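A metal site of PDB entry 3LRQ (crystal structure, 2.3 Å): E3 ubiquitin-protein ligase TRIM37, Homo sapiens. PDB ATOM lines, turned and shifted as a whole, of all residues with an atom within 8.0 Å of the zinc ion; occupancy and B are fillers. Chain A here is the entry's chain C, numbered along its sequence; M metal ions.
The side-chain sulfur (SG) of Cys 46 sits close to the backbone NH (N) of Arg 33 (3.6 Å).
SG of Cys 28 sits close to N of Glu 30 (3.2 Å).
SG of Cys 25 sits close to N of Ile 27 (3.3 Å).
The side-chain sulfur (SG) of Cys 25 lies close to the side-chain sulfur (SG) of Cys 45 (3.5 Å).
The backbone NH (N) of Cys 25 is in hydrogen-bond range of the backbone carbonyl oxygen (O) of Glu 30 (2.7 Å).
Four residues have an atom within 4 Å of the zinc ion: Cys 25, Cys 28, Cys 46 and Cys 49.
The nearest printed residue that does not touch the zinc ion is Ile 27 (4.9 Å).
The zinc ion is bound by the side-chain sulfur (SG) of Cys 46, the side-chain sulfur (SG) of Cys 49, the side-chain sulfur (SG) of Cys 28 and the side-chain sulfur (SG) of Cys 25.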
ATOM      1  N   ARG A  24      31.899   6.304  21.876  1.00  0.00           N
ATOM      2  CA  ARG A  24      30.655   5.943  22.535  1.00  0.00           C
ATOM      3  C   ARG A  24      30.205   4.604  22.011  1.00  0.00           C
ATOM      4  O   ARG A  24      30.336   4.306  20.816  1.00  0.00           O
ATOM      5  CB  ARG A  24      29.567   6.994  22.318  1.00  0.00           C
ATOM      6  CG  ARG A  24      29.670   8.169  23.261  1.00  0.00           C
ATOM      7  CD  ARG A  24      28.497   9.108  23.113  1.00  0.00           C
ATOM      8  NE  ARG A  24      28.899  10.465  23.461  1.00  0.00           N
ATOM      9  CZ  ARG A  24      29.314  11.368  22.585  1.00  0.00           C
ATOM     10  NH1 ARG A  24      29.358  11.063  21.293  1.00  0.00           N
ATOM     11  NH2 ARG A  24      29.678  12.575  22.980  1.00  0.00           N
ATOM     12  N   CYS A  25      29.680   3.783  22.915  1.00  0.00           N
ATOM     13  CA  CYS A  25      29.151   2.500  22.531  1.00  0.00           C
ATOM     14  C   CYS A  25      28.049   2.735  21.522  1.00  0.00           C
ATOM     15  O   CYS A  25      27.172   3.579  21.750  1.00  0.00           O
ATOM     16  CB  CYS A  25      28.615   1.761  23.755  1.00  0.00           C
ATOM     17  SG  CYS A  25      27.623   0.298  23.344  1.00  0.00           S
ATOM     18  N   PHE A  26      28.100   2.012  20.397  1.00  0.00           N
ATOM     19  CA  PHE A  26      27.114   2.182  19.336  1.00  0.00           C
ATOM     20  C   PHE A  26      25.761   1.561  19.628  1.00  0.00           C
ATOM     21  O   PHE A  26      24.809   1.787  18.892  1.00  0.00           O
ATOM     22  CB  PHE A  26      27.627   1.645  17.995  1.00  0.00           C
ATOM     23  CG  PHE A  26      28.047   0.206  18.028  1.00  0.00           C
ATOM     24  CD1 PHE A  26      27.109  -0.810  17.999  1.00  0.00           C
ATOM     25  CD2 PHE A  26      29.391  -0.123  18.045  1.00  0.00           C
ATOM     26  CE1 PHE A  26      27.510  -2.131  18.012  1.00  0.00           C
ATOM     27  CE2 PHE A  26      29.787  -1.456  18.051  1.00  0.00           C
ATOM     28  CZ  PHE A  26      28.847  -2.461  18.035  1.00  0.00           C
ATOM     29  N   ILE A  27      25.673   0.769  20.692  1.00  0.00           N
ATOM     30  CA  ILE A  27      24.399   0.210  21.119  1.00  0.00           C
ATOM     31  C   ILE A  27      23.740   1.136  22.150  1.00  0.00           C
ATOM     32  O   ILE A  27      22.690   1.712  21.895  1.00  0.00           O
ATOM     33  CB  ILE A  27      24.578  -1.205  21.738  1.00  0.00           C
ATOM     34  CG1 ILE A  27      24.984  -2.211  20.662  1.00  0.00           C
ATOM     35  CG2 ILE A  27      23.306  -1.656  22.439  1.00  0.00           C
ATOM     36  CD1 ILE A  27      25.134  -3.630  21.174  1.00  0.00           C
ATOM     37  N   CYS A  28      24.373   1.294  23.314  1.00  0.00           N
ATOM     38  CA  CYS A  28      23.784   2.071  24.407  1.00  0.00           C
ATOM     39  C   CYS A  28      23.958   3.600  24.276  1.00  0.00           C
ATOM     40  O   CYS A  28      23.320   4.356  24.998  1.00  0.00           O
ATOM     41  CB  CYS A  28      24.330   1.603  25.752  1.00  0.00           C
ATOM     42  SG  CYS A  28      25.979   2.312  26.154  1.00  0.00           S
ATOM     43  N   MET A  29      24.843   4.034  23.381  1.00  0.00           N
ATOM     44  CA  MET A  29      25.062   5.466  23.148  1.00  0.00           C
ATOM     45  C   MET A  29      25.844   6.112  24.290  1.00  0.00           C
ATOM     46  O   MET A  29      25.953   7.341  24.354  1.00  0.00           O
ATOM     47  CB  MET A  29      23.739   6.225  22.965  1.00  0.00           C
ATOM     48  CG  MET A  29      22.777   5.577  21.982  1.00  0.00           C
ATOM     49  SD  MET A  29      23.641   5.202  20.286  1.00  0.00           S
ATOM     50  CE  MET A  29      24.414   6.972  19.943  1.00  0.00           C
ATOM     51  N   GLU A  30      26.386   5.305  25.176  1.00  0.00           N
ATOM     52  CA  GLU A  30      27.113   5.865  26.316  1.00  0.00           C
ATOM     53  C   GLU A  30      28.624   5.727  26.161  1.00  0.00           C
ATOM     54  O   GLU A  30      29.095   5.141  25.178  1.00  0.00           O
ATOM     55  CB  GLU A  30      26.663   5.212  27.621  1.00  0.00           C
ATOM     56  CG  GLU A  30      25.167   5.344  27.912  1.00  0.00           C
ATOM     57  CD  GLU A  30      24.821   6.643  28.623  1.00  0.00           C
ATOM     58  OE1 GLU A  30      25.508   6.983  29.625  1.00  0.00           O
ATOM     59  OE2 GLU A  30      23.862   7.322  28.186  1.00  0.00           O
ATOM     60  N   LYS A  31      29.364   6.260  27.119  1.00  0.00           N
ATOM     61  CA  LYS A  31      30.810   6.086  27.178  1.00  0.00           C
ATOM     62  C   LYS A  31      31.136   4.608  27.315  1.00  0.00           C
ATOM     63  O   LYS A  31      30.391   3.858  27.942  1.00  0.00           O
ATOM     64  CB  LYS A  31      31.388   6.810  28.392  1.00  0.00           C
ATOM     65  CG  LYS A  31      32.026   8.146  28.088  1.00  0.00           C
ATOM     66  CD  LYS A  31      32.746   8.654  29.325  1.00  0.00           C
ATOM     67  CE  LYS A  31      32.581   7.662  30.481  1.00  0.00           C
ATOM     68  NZ  LYS A  31      33.777   7.546  31.372  1.00  0.00           N
ATOM     69  N   LEU A  32      32.259   4.177  26.736  1.00  0.00           N
ATOM     70  CA  LEU A  32      32.559   2.760  26.709  1.00  0.00           C
ATOM     71  C   LEU A  32      32.878   2.202  28.083  1.00  0.00           C
ATOM     72  O   LEU A  32      33.645   2.778  28.847  1.00  0.00           O
ATOM     73  CB  LEU A  32      33.704   2.455  25.736  1.00  0.00           C
ATOM     74  CG  LEU A  32      33.374   2.576  24.238  1.00  0.00           C
ATOM     75  CD1 LEU A  32      34.669   2.453  23.435  1.00  0.00           C
ATOM     76  CD2 LEU A  32      32.361   1.532  23.794  1.00  0.00           C
ATOM     77  N   ARG A  33      32.267   1.072  28.406  1.00  0.00           N
ATOM     78  CA  ARG A  33      32.653   0.372  29.613  1.00  0.00           C
ATOM     79  C   ARG A  33      33.035  -1.040  29.242  1.00  0.00           C
ATOM     80  O   ARG A  33      32.172  -1.825  28.819  1.00  0.00           O
ATOM     81  CB  ARG A  33      31.529   0.382  30.636  1.00  0.00           C
ATOM     82  CG  ARG A  33      31.764  -0.550  31.791  1.00  0.00           C
ATOM     83  CD  ARG A  33      31.462   0.174  33.085  1.00  0.00           C
ATOM     84  NE  ARG A  33      31.253  -0.768  34.177  1.00  0.00           N
ATOM     85  CZ  ARG A  33      30.151  -1.479  34.329  1.00  0.00           C
ATOM     86  NH1 ARG A  33      29.163  -1.372  33.445  1.00  0.00           N
ATOM     87  NH2 ARG A  33      30.019  -2.309  35.359  1.00  0.00           N
ATOM     88  N   LEU A  44      33.037   0.247  18.114  1.00  0.00           N
ATOM     89  CA  LEU A  44      33.198  -0.112  19.524  1.00  0.00           C
ATOM     90  C   LEU A  44      31.880  -0.175  20.314  1.00  0.00           C
ATOM     91  O   LEU A  44      31.009   0.681  20.143  1.00  0.00           O
ATOM     92  CB  LEU A  44      34.139   0.879  20.217  1.00  0.00           C
ATOM     93  CG  LEU A  44      35.542   1.049  19.601  1.00  0.00           C
ATOM     94  CD1 LEU A  44      36.121   2.396  19.982  1.00  0.00           C
ATOM     95  CD2 LEU A  44      36.446  -0.066  20.075  1.00  0.00           C
ATOM     96  N   CYS A  45      31.780  -1.167  21.197  1.00  0.00           N
ATOM     97  CA  CYS A  45      30.567  -1.464  21.966  1.00  0.00           C
ATOM     98  C   CYS A  45      30.996  -1.867  23.375  1.00  0.00           C
ATOM     99  O   CYS A  45      32.081  -2.459  23.549  1.00  0.00           O
ATOM    100  CB  CYS A  45      29.827  -2.633  21.316  1.00  0.00           C
ATOM    101  SG  CYS A  45      28.133  -2.848  21.861  1.00  0.00           S
ATOM    102  N   CYS A  46      30.194  -1.533  24.389  1.00  0.00           N
ATOM    103  CA  CYS A  46      30.442  -2.081  25.744  1.00  0.00           C
ATOM    104  C   CYS A  46      30.393  -3.616  25.684  1.00  0.00           C
ATOM    105  O   CYS A  46      29.632  -4.173  24.912  1.00  0.00           O
ATOM    106  CB  CYS A  46      29.372  -1.615  26.728  1.00  0.00           C
ATOM    107  SG  CYS A  46      29.165   0.171  26.819  1.00  0.00           S
ATOM    108  N   PHE A  47      31.205  -4.294  26.482  1.00  0.00           N
ATOM    109  CA  PHE A  47      31.166  -5.753  26.480  1.00  0.00           C
ATOM    110  C   PHE A  47      29.755  -6.245  26.799  1.00  0.00           C
ATOM    111  O   PHE A  47      29.207  -7.116  26.112  1.00  0.00           O
ATOM    112  CB  PHE A  47      32.180  -6.308  27.493  1.00  0.00           C
ATOM    113  CG  PHE A  47      32.435  -7.781  27.355  1.00  0.00           C
ATOM    114  CD1 PHE A  47      31.876  -8.505  26.326  1.00  0.00           C
ATOM    115  CD2 PHE A  47      33.260  -8.446  28.273  1.00  0.00           C
ATOM    116  CE1 PHE A  47      32.126  -9.867  26.184  1.00  0.00           C
ATOM    117  CE2 PHE A  47      33.516  -9.806  28.152  1.00  0.00           C
ATOM    118  CZ  PHE A  47      32.950 -10.522  27.101  1.00  0.00           C
ATOM    119  N   SER A  48      29.141  -5.679  27.832  1.00  0.00           N
ATOM    120  CA  SER A  48      27.804  -6.113  28.264  1.00  0.00           C
ATOM    121  C   SER A  48      26.759  -5.920  27.183  1.00  0.00           C
ATOM    122  O   SER A  48      25.923  -6.794  26.955  1.00  0.00           O
ATOM    123  CB  SER A  48      27.366  -5.366  29.511  1.00  0.00           C
ATOM    124  OG  SER A  48      28.204  -5.699  30.599  1.00  0.00           O
ATOM    125  N   CYS A  49      26.795  -4.761  26.515  1.00  0.00           N
ATOM    126  CA  CYS A  49      25.777  -4.457  25.512  1.00  0.00           C
ATOM    127  C   CYS A  49      25.809  -5.474  24.391  1.00  0.00           C
ATOM    128  O   CYS A  49      24.794  -6.073  24.055  1.00  0.00           O
ATOM    129  CB  CYS A  49      25.945  -3.052  24.950  1.00  0.00           C
ATOM    130  SG  CYS A  49      25.887  -1.800  26.225  1.00  0.00           S
ATOM    131  N   ILE A  50      26.994  -5.685  23.825  1.00  0.00           N
ATOM    132  CA  ILE A  50      27.109  -6.621  22.724  1.00  0.00           C
ATOM    133  C   ILE A  50      26.741  -8.036  23.180  1.00  0.00           C
ATOM    134  O   ILE A  50      26.122  -8.808  22.444  1.00  0.00           O
ATOM    135  CB  ILE A  50      28.516  -6.580  22.034  1.00  0.00           C
ATOM    136  CG1 ILE A  50      28.513  -7.377  20.727  1.00  0.00           C
ATOM    137  CG2 ILE A  50      29.645  -6.995  23.026  1.00  0.00           C
ATOM    138  CD1 ILE A  50      27.341  -7.053  19.776  1.00  0.00           C
HETATM  139 ZN    ZN M   1      27.062   0.207  25.736  1.00  0.00          ZN
